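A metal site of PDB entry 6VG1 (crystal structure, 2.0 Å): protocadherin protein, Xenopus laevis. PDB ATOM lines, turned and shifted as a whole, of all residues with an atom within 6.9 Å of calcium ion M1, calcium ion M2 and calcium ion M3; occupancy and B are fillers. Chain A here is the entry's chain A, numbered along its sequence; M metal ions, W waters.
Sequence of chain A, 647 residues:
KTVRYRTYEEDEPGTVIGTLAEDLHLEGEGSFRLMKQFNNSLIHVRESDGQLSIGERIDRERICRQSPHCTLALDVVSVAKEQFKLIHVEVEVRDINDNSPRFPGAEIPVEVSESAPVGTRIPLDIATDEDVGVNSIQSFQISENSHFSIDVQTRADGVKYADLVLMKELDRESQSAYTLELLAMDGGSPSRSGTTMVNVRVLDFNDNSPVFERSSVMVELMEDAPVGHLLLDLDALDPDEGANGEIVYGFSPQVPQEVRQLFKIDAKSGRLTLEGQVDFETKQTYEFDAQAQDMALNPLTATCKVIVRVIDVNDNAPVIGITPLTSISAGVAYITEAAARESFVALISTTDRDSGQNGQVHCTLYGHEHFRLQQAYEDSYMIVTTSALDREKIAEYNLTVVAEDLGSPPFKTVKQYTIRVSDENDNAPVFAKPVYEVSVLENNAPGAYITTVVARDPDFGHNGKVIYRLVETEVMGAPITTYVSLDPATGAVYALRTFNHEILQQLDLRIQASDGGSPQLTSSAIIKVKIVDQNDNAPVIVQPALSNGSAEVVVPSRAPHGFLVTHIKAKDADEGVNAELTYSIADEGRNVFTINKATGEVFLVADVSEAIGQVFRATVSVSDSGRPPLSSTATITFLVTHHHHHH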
ATOM      1  N   GLU A 223      -3.735  -6.501  10.903  1.00  0.00           N
ATOM      2  CA  GLU A 223      -4.145  -7.901  10.938  1.00  0.00           C
ATOM      3  C   GLU A 223      -3.070  -8.801  11.541  1.00  0.00           C
ATOM      4  O   GLU A 223      -3.344  -9.979  11.818  1.00  0.00           O
ATOM      5  CB  GLU A 223      -4.523  -8.420   9.544  1.00  0.00           C
ATOM      6  CG  GLU A 223      -3.436  -8.584   8.539  1.00  0.00           C
ATOM      7  CD  GLU A 223      -3.874  -9.420   7.330  1.00  0.00           C
ATOM      8  OE1 GLU A 223      -4.532 -10.472   7.539  1.00  0.00           O
ATOM      9  OE2 GLU A 223      -3.590  -9.026   6.171  1.00  0.00           O
ATOM     10  N   VAL A 278      -6.700 -11.950  14.136  1.00  0.00           N
ATOM     11  CA  VAL A 278      -7.614 -11.573  13.078  1.00  0.00           C
ATOM     12  C   VAL A 278      -6.927 -11.840  11.743  1.00  0.00           C
ATOM     13  O   VAL A 278      -5.716 -12.053  11.659  1.00  0.00           O
ATOM     14  CB  VAL A 278      -8.047 -10.086  13.188  1.00  0.00           C
ATOM     15  CG1 VAL A 278      -8.863  -9.856  14.435  1.00  0.00           C
ATOM     16  CG2 VAL A 278      -6.832  -9.165  13.152  1.00  0.00           C
ATOM     17  N   ASP A 279      -7.721 -11.843  10.668  1.00  0.00           N
ATOM     18  CA  ASP A 279      -7.191 -12.121   9.338  1.00  0.00           C
ATOM     19  C   ASP A 279      -7.968 -11.294   8.334  1.00  0.00           C
ATOM     20  O   ASP A 279      -9.134 -11.588   8.040  1.00  0.00           O
ATOM     21  CB  ASP A 279      -7.302 -13.610   9.011  1.00  0.00           C
ATOM     22  CG  ASP A 279      -6.839 -13.921   7.624  1.00  0.00           C
ATOM     23  OD1 ASP A 279      -6.204 -13.058   6.983  1.00  0.00           O
ATOM     24  OD2 ASP A 279      -7.110 -15.057   7.153  1.00  0.00           O
ATOM     25  N   PHE A 280      -7.311 -10.264   7.779  1.00  0.00           N
ATOM     26  CA  PHE A 280      -7.985  -9.354   6.860  1.00  0.00           C
ATOM     27  C   PHE A 280      -8.605 -10.111   5.699  1.00  0.00           C
ATOM     28  O   PHE A 280      -9.680  -9.751   5.212  1.00  0.00           O
ATOM     29  CB  PHE A 280      -6.975  -8.319   6.359  1.00  0.00           C
ATOM     30  CG  PHE A 280      -7.543  -7.337   5.391  1.00  0.00           C
ATOM     31  CD1 PHE A 280      -8.020  -6.124   5.829  1.00  0.00           C
ATOM     32  CD2 PHE A 280      -7.603  -7.637   4.055  1.00  0.00           C
ATOM     33  CE1 PHE A 280      -8.548  -5.214   4.943  1.00  0.00           C
ATOM     34  CE2 PHE A 280      -8.126  -6.730   3.157  1.00  0.00           C
ATOM     35  CZ  PHE A 280      -8.600  -5.511   3.602  1.00  0.00           C
ATOM     36  N   GLU A 281      -7.936 -11.150   5.211  1.00  0.00           N
ATOM     37  CA  GLU A 281      -8.470 -11.902   4.085  1.00  0.00           C
ATOM     38  C   GLU A 281      -9.703 -12.715   4.432  1.00  0.00           C
ATOM     39  O   GLU A 281     -10.270 -13.341   3.531  1.00  0.00           O
ATOM     40  CB  GLU A 281      -7.402 -12.841   3.525  1.00  0.00           C
ATOM     41  CG  GLU A 281      -6.337 -12.141   2.731  1.00  0.00           C
ATOM     42  CD  GLU A 281      -5.445 -11.299   3.612  1.00  0.00           C
ATOM     43  OE1 GLU A 281      -5.153 -11.721   4.768  1.00  0.00           O
ATOM     44  OE2 GLU A 281      -5.039 -10.209   3.141  1.00  0.00           O
ATOM     45  N   THR A 282     -10.117 -12.734   5.694  1.00  0.00           N
ATOM     46  CA  THR A 282     -11.264 -13.505   6.139  1.00  0.00           C
ATOM     47  C   THR A 282     -12.399 -12.616   6.614  1.00  0.00           C
ATOM     48  O   THR A 282     -13.557 -12.818   6.248  1.00  0.00           O
ATOM     49  CB  THR A 282     -10.859 -14.457   7.277  1.00  0.00           C
ATOM     50  OG1 THR A 282      -9.838 -15.344   6.808  1.00  0.00           O
ATOM     51  CG2 THR A 282     -12.049 -15.258   7.757  1.00  0.00           C
ATOM     52  N   ILE A 311      -6.689  -3.917   9.084  1.00  0.00           N
ATOM     53  CA  ILE A 311      -5.850  -3.360   8.029  1.00  0.00           C
ATOM     54  C   ILE A 311      -5.036  -4.476   7.399  1.00  0.00           C
ATOM     55  O   ILE A 311      -4.460  -5.308   8.106  1.00  0.00           O
ATOM     56  CB  ILE A 311      -4.933  -2.250   8.566  1.00  0.00           C
ATOM     57  CG1 ILE A 311      -5.779  -1.066   9.036  1.00  0.00           C
ATOM     58  CG2 ILE A 311      -3.936  -1.851   7.505  1.00  0.00           C
ATOM     59  CD1 ILE A 311      -6.138  -1.155  10.478  1.00  0.00           C
ATOM     60  N   ASP A 312      -4.934  -4.453   6.075  1.00  0.00           N
ATOM     61  CA  ASP A 312      -4.328  -5.556   5.344  1.00  0.00           C
ATOM     62  C   ASP A 312      -2.813  -5.510   5.420  1.00  0.00           C
ATOM     63  O   ASP A 312      -2.204  -4.447   5.322  1.00  0.00           O
ATOM     64  CB  ASP A 312      -4.771  -5.504   3.882  1.00  0.00           C
ATOM     65  CG  ASP A 312      -4.136  -6.590   3.038  1.00  0.00           C
ATOM     66  OD1 ASP A 312      -3.581  -7.549   3.616  1.00  0.00           O
ATOM     67  OD2 ASP A 312      -4.196  -6.477   1.787  1.00  0.00           O
ATOM     68  N   VAL A 313      -2.221  -6.680   5.603  1.00  0.00           N
ATOM     69  CA  VAL A 313      -0.763  -6.831   5.601  1.00  0.00           C
ATOM     70  C   VAL A 313      -0.374  -7.754   4.461  1.00  0.00           C
ATOM     71  O   VAL A 313      -1.148  -8.640   4.072  1.00  0.00           O
ATOM     72  CB  VAL A 313      -0.248  -7.379   6.941  1.00  0.00           C
ATOM     73  CG1 VAL A 313       1.250  -7.621   6.854  1.00  0.00           C
ATOM     74  CG2 VAL A 313      -0.563  -6.407   8.046  1.00  0.00           C
ATOM     75  N   ASN A 314       0.822  -7.555   3.922  1.00  0.00           N
ATOM     76  CA  ASN A 314       1.300  -8.410   2.832  1.00  0.00           C
ATOM     77  C   ASN A 314       1.731  -9.728   3.451  1.00  0.00           C
ATOM     78  O   ASN A 314       2.918 -10.000   3.666  1.00  0.00           O
ATOM     79  CB  ASN A 314       2.417  -7.768   2.041  1.00  0.00           C
ATOM     80  CG  ASN A 314       2.628  -8.454   0.709  1.00  0.00           C
ATOM     81  OD1 ASN A 314       1.722  -9.103   0.192  1.00  0.00           O
ATOM     82  ND2 ASN A 314       3.821  -8.300   0.140  1.00  0.00           N
ATOM     83  N   ASP A 315       0.737 -10.574   3.749  1.00  0.00           N
ATOM     84  CA  ASP A 315       0.975 -11.863   4.368  1.00  0.00           C
ATOM     85  C   ASP A 315       0.618 -13.022   3.434  1.00  0.00           C
ATOM     86  O   ASP A 315       0.495 -14.166   3.884  1.00  0.00           O
ATOM     87  CB  ASP A 315       0.209 -11.979   5.684  1.00  0.00           C
ATOM     88  CG  ASP A 315      -1.298 -11.797   5.521  1.00  0.00           C
ATOM     89  OD1 ASP A 315      -1.754 -11.214   4.513  1.00  0.00           O
ATOM     90  OD2 ASP A 315      -2.015 -12.242   6.425  1.00  0.00           O
ATOM     91  N   ASN A 316       0.490 -12.740   2.140  1.00  0.00           N
ATOM     92  CA  ASN A 316       0.294 -13.788   1.148  1.00  0.00           C
ATOM     93  C   ASN A 316       1.206 -13.540  -0.042  1.00  0.00           C
ATOM     94  O   ASN A 316       1.444 -12.394  -0.427  1.00  0.00           O
ATOM     95  CB  ASN A 316      -1.159 -13.850   0.649  1.00  0.00           C
ATOM     96  CG  ASN A 316      -2.106 -14.428   1.688  1.00  0.00           C
ATOM     97  OD1 ASN A 316      -2.321 -15.649   1.745  1.00  0.00           O
ATOM     98  ND2 ASN A 316      -2.654 -13.560   2.517  1.00  0.00           N
ATOM     99  N   ALA A 317       1.690 -14.619  -0.637  1.00  0.00           N
ATOM    100  CA  ALA A 317       2.482 -14.555  -1.844  1.00  0.00           C
ATOM    101  C   ALA A 317       1.638 -14.942  -3.037  1.00  0.00           C
ATOM    102  O   ALA A 317       0.564 -15.517  -2.883  1.00  0.00           O
ATOM    103  CB  ALA A 317       3.693 -15.478  -1.746  1.00  0.00           C
ATOM    104  N   PRO A 318       2.086 -14.614  -4.248  1.00  0.00           N
ATOM    105  CA  PRO A 318       1.339 -15.046  -5.436  1.00  0.00           C
ATOM    106  C   PRO A 318       1.258 -16.556  -5.563  1.00  0.00           C
ATOM    107  O   PRO A 318       2.198 -17.285  -5.217  1.00  0.00           O
ATOM    108  CB  PRO A 318       2.131 -14.435  -6.596  1.00  0.00           C
ATOM    109  CG  PRO A 318       2.771 -13.218  -5.978  1.00  0.00           C
ATOM    110  CD  PRO A 318       3.110 -13.600  -4.555  1.00  0.00           C
ATOM    111  N   ASP A 352      -3.159 -13.269  -5.724  1.00  0.00           N
ATOM    112  CA  ASP A 352      -2.597 -12.858  -4.435  1.00  0.00           C
ATOM    113  C   ASP A 352      -3.767 -12.561  -3.518  1.00  0.00           C
ATOM    114  O   ASP A 352      -4.596 -11.712  -3.835  1.00  0.00           O
ATOM    115  CB  ASP A 352      -1.696 -11.624  -4.574  1.00  0.00           C
ATOM    116  CG  ASP A 352      -0.806 -11.384  -3.347  1.00  0.00           C
ATOM    117  OD1 ASP A 352       0.437 -11.446  -3.493  1.00  0.00           O
ATOM    118  OD2 ASP A 352      -1.340 -11.098  -2.243  1.00  0.00           O
ATOM    119  N   ARG A 353      -3.849 -13.264  -2.380  1.00  0.00           N
ATOM    120  CA  ARG A 353      -5.003 -13.133  -1.497  1.00  0.00           C
ATOM    121  C   ARG A 353      -5.132 -11.724  -0.916  1.00  0.00           C
ATOM    122  O   ARG A 353      -6.221 -11.360  -0.453  1.00  0.00           O
ATOM    123  CB  ARG A 353      -4.910 -14.102  -0.300  1.00  0.00           C
ATOM    124  CG  ARG A 353      -4.783 -15.571  -0.652  1.00  0.00           C
ATOM    125  CD  ARG A 353      -6.157 -16.171  -0.905  1.00  0.00           C
ATOM    126  NE  ARG A 353      -6.999 -16.153   0.292  1.00  0.00           N
ATOM    127  CZ  ARG A 353      -8.285 -16.442   0.280  1.00  0.00           C
ATOM    128  NH1 ARG A 353      -8.870 -16.757  -0.868  1.00  0.00           N
ATOM    129  NH2 ARG A 353      -8.998 -16.408   1.399  1.00  0.00           N
ATOM    130  N   ASP A 354      -4.038 -10.970  -0.850  1.00  0.00           N
ATOM    131  CA  ASP A 354      -4.096  -9.667  -0.209  1.00  0.00           C
ATOM    132  C   ASP A 354      -4.848  -8.666  -1.096  1.00  0.00           C
ATOM    133  O   ASP A 354      -5.376  -8.990  -2.163  1.00  0.00           O
ATOM    134  CB  ASP A 354      -2.688  -9.135   0.073  1.00  0.00           C
ATOM    135  CG  ASP A 354      -1.867 -10.096   0.893  1.00  0.00           C
ATOM    136  OD1 ASP A 354      -2.343 -10.530   1.974  1.00  0.00           O
ATOM    137  OD2 ASP A 354      -0.737 -10.417   0.463  1.00  0.00           O
ATOM    138  N   SER A 355      -4.856  -7.412  -0.654  1.00  0.00           N
ATOM    139  CA  SER A 355      -5.530  -6.313  -1.340  1.00  0.00           C
ATOM    140  C   SER A 355      -4.559  -5.167  -1.590  1.00  0.00           C
ATOM    141  O   SER A 355      -3.458  -5.106  -1.032  1.00  0.00           O
ATOM    142  CB  SER A 355      -6.725  -5.814  -0.520  1.00  0.00           C
ATOM    143  OG  SER A 355      -7.696  -6.828  -0.398  1.00  0.00           O
ATOM    144  N   GLN A 357      -1.838  -2.786  -3.530  1.00  0.00           N
ATOM    145  CA  GLN A 357      -0.565  -3.169  -4.140  1.00  0.00           C
ATOM    146  C   GLN A 357      -0.096  -4.526  -3.646  1.00  0.00           C
ATOM    147  O   GLN A 357       0.529  -5.281  -4.403  1.00  0.00           O
ATOM    148  CB  GLN A 357       0.496  -2.118  -3.824  1.00  0.00           C
ATOM    149  CG  GLN A 357       0.228  -0.736  -4.387  1.00  0.00           C
ATOM    150  CD  GLN A 357       0.742  -0.564  -5.799  1.00  0.00           C
ATOM    151  OE1 GLN A 357       1.884  -0.911  -6.109  1.00  0.00           O
ATOM    152  NE2 GLN A 357      -0.105  -0.042  -6.676  1.00  0.00           N
ATOM    153  N   ASN A 358      -0.381  -4.848  -2.386  1.00  0.00           N
ATOM    154  CA  ASN A 358       0.073  -6.112  -1.829  1.00  0.00           C
ATOM    155  C   ASN A 358      -0.576  -7.295  -2.536  1.00  0.00           C
ATOM    156  O   ASN A 358      -0.010  -8.398  -2.501  1.00  0.00           O
ATOM    157  CB  ASN A 358      -0.219  -6.167  -0.330  1.00  0.00           C
ATOM    158  CG  ASN A 358       0.568  -5.134   0.449  1.00  0.00           C
ATOM    159  OD1 ASN A 358       1.655  -4.735   0.050  1.00  0.00           O
ATOM    160  ND2 ASN A 358       0.039  -4.741   1.599  1.00  0.00           N
ATOM    161  N   GLY A 359      -1.721  -7.089  -3.194  1.00  0.00           N
ATOM    162  CA  GLY A 359      -2.407  -8.156  -3.887  1.00  0.00           C
ATOM    163  C   GLY A 359      -2.345  -8.083  -5.393  1.00  0.00           C
ATOM    164  O   GLY A 359      -3.014  -8.866  -6.063  1.00  0.00           O
ATOM    165  N   GLN A 360      -1.565  -7.165  -5.952  1.00  0.00           N
ATOM    166  CA  GLN A 360      -1.508  -6.933  -7.384  1.00  0.00           C
ATOM    167  C   GLN A 360      -0.297  -7.654  -7.935  1.00  0.00           C
ATOM    168  O   GLN A 360       0.822  -7.474  -7.435  1.00  0.00           O
ATOM    169  CB  GLN A 360      -1.416  -5.435  -7.642  1.00  0.00           C
ATOM    170  CG  GLN A 360      -1.713  -5.024  -9.035  1.00  0.00           C
ATOM    171  CD  GLN A 360      -2.024  -3.539  -9.092  1.00  0.00           C
ATOM    172  OE1 GLN A 360      -2.843  -3.035  -8.328  1.00  0.00           O
ATOM    173  NE2 GLN A 360      -1.368  -2.832  -9.997  1.00  0.00           N
ATOM    174  N   VAL A 361      -0.503  -8.464  -8.976  1.00  0.00           N
ATOM    175  CA  VAL A 361       0.516  -9.394  -9.449  1.00  0.00           C
ATOM    176  C   VAL A 361       0.994  -9.012 -10.842  1.00  0.00           C
ATOM    177  O   VAL A 361       0.194  -8.672 -11.724  1.00  0.00           O
ATOM    178  CB  VAL A 361       0.002 -10.843  -9.461  1.00  0.00           C
ATOM    179  CG1 VAL A 361      -0.424 -11.266  -8.080  1.00  0.00           C
ATOM    180  CG2 VAL A 361      -1.164 -10.989 -10.454  1.00  0.00           C
ATOM    181  N   ASP A 405       4.193  -9.711  -6.455  1.00  0.00           N
ATOM    182  CA  ASP A 405       3.208  -8.718  -6.041  1.00  0.00           C
ATOM    183  C   ASP A 405       3.913  -7.362  -5.913  1.00  0.00           C
ATOM    184  O   ASP A 405       5.135  -7.250  -6.095  1.00  0.00           O
ATOM    185  CB  ASP A 405       2.482  -9.145  -4.745  1.00  0.00           C
ATOM    186  CG  ASP A 405       3.321  -9.013  -3.496  1.00  0.00           C
ATOM    187  OD1 ASP A 405       4.444  -8.451  -3.564  1.00  0.00           O
ATOM    188  OD2 ASP A 405       2.849  -9.495  -2.432  1.00  0.00           O
ATOM    189  N   LEU A 406       3.147  -6.318  -5.606  1.00  0.00           N
ATOM    190  CA  LEU A 406       3.689  -4.969  -5.527  1.00  0.00           C
ATOM    191  C   LEU A 406       3.830  -4.505  -4.082  1.00  0.00           C
ATOM    192  O   LEU A 406       3.784  -3.306  -3.807  1.00  0.00           O
ATOM    193  CB  LEU A 406       2.831  -4.004  -6.326  1.00  0.00           C
ATOM    194  CG  LEU A 406       3.127  -3.899  -7.812  1.00  0.00           C
ATOM    195  CD1 LEU A 406       4.486  -3.208  -8.027  1.00  0.00           C
ATOM    196  CD2 LEU A 406       3.135  -5.251  -8.529  1.00  0.00           C
ATOM    197  N   GLY A 407       4.046  -5.435  -3.161  1.00  0.00           N
ATOM    198  CA  GLY A 407       4.338  -5.070  -1.791  1.00  0.00           C
ATOM    199  C   GLY A 407       5.728  -4.469  -1.661  1.00  0.00           C
ATOM    200  O   GLY A 407       6.521  -4.419  -2.584  1.00  0.00           O
ATOM    201  N   PHE A 411       6.611 -10.120  -2.567  1.00  0.00           N
ATOM    202  CA  PHE A 411       6.696 -11.578  -2.616  1.00  0.00           C
ATOM    203  C   PHE A 411       6.893 -11.998  -4.057  1.00  0.00           C
ATOM    204  O   PHE A 411       6.265 -11.443  -4.964  1.00  0.00           O
ATOM    205  CB  PHE A 411       5.424 -12.226  -2.058  1.00  0.00           C
ATOM    206  CG  PHE A 411       5.461 -12.503  -0.557  1.00  0.00           C
ATOM    207  CD1 PHE A 411       6.270 -13.516  -0.056  1.00  0.00           C
ATOM    208  CD2 PHE A 411       4.677 -11.766   0.329  1.00  0.00           C
ATOM    209  CE1 PHE A 411       6.302 -13.771   1.313  1.00  0.00           C
ATOM    210  CE2 PHE A 411       4.717 -12.020   1.669  1.00  0.00           C
ATOM    211  CZ  PHE A 411       5.514 -13.021   2.178  1.00  0.00           C
HETATM  212 CA    CA M   1       0.749 -10.299  -1.496  1.00  0.00          CA
HETATM  213 CA    CA M   2      -3.184  -9.646   3.961  1.00  0.00          CA
HETATM  214 CA    CA M   3      -4.022 -12.653   6.613  1.00  0.00          CA
HETATM  215  O   HOH W   1      -3.807 -13.954   8.626  1.00  0.00           O
HETATM  216  O   HOH W   2      -3.639 -14.602   5.433  1.00  0.00           O
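O of Asn 358 is bound to calcium ion M1 (2.3 Å). OD1 of Asn 314 is bound to calcium ion M1 (2.3 Å). Calcium ion M1 is bound by the side-chain carboxylate (OD1) of Asp 352 (2.3 Å). Calcium ion M1 is bound by OD2 of Asp 352 (2.4 Å). Calcium ion M1 is bound by OD2 of Asp 405. O of Asn 316 is bound to calcium ion M1. OD2 of Asp 354 binds calcium ion M1 (2.5 Å).
Six residues have an atom within 4 Å of calcium ion M2: Glu 223, Glu 281, Asp 312, Val 313, Asp 315 and Asp 354. The nearest printed residue that does not touch calcium ion M2 is Asn 316 (4.2 Å).
Calcium ion M2 is bound by the side-chain carboxylate (OE2) of Glu 281, the side-chain carboxylate (OD1) of Asp 312, the side-chain carboxylate (OD1) of Asp 315, the backbone carbonyl oxygen (O) of Val 313, the side-chain carboxylate (OD1) of Asp 354 and the side-chain carboxylate (OE2) of Glu 223. Calcium ion M2 has six donor atoms within binding distance. Slightly farther from calcium ion M2 lies the side-chain carboxylate (OE1) of Glu 281 (3.0 Å).
Of the 27 residues printed, 6 come within 4 Å of calcium ion M1. The nearest printed residue that does not touch calcium ion M1 is Gly 359 (4.4 Å).
Calcium ion M3 is bound by the side-chain carboxylate of Asp 315, the side-chain carboxylate of Asp 279, water W2, the side-chain carboxylate of Glu 281, water W1 and the side-chain carboxylate of Glu 223. Calcium ion M3 has six donor atoms within binding distance.
The side-chain carboxylate of Asp 405 sits at hydrogen-bond distance from the backbone NH of Gly 407 (3.1 Å). The side-chain carboxylate of Asp 315 sits close to the side-chain amide nitrogen of Asn 316, at 3.2 Å. The side-chain carboxylate of Asp 312 lies within hydrogen-bond range of the backbone NH of Ser 355 (2.7 Å). The side-chain carboxylate (OE1) of Glu 223 sits close to the backbone NH (N) of Phe 280. The side-chain carboxylate (OD1) of Asp 405 lies within hydrogen-bond range of the backbone NH (N) of Phe 411 (2.9 Å). OD2 of Asp 279 lies within hydrogen-bond range of OG1 of Thr 282 (2.8 Å). The backbone carbonyl oxygen of Ile 311 lies within hydrogen-bond range of the backbone NH of Glu 223 (3.1 Å).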
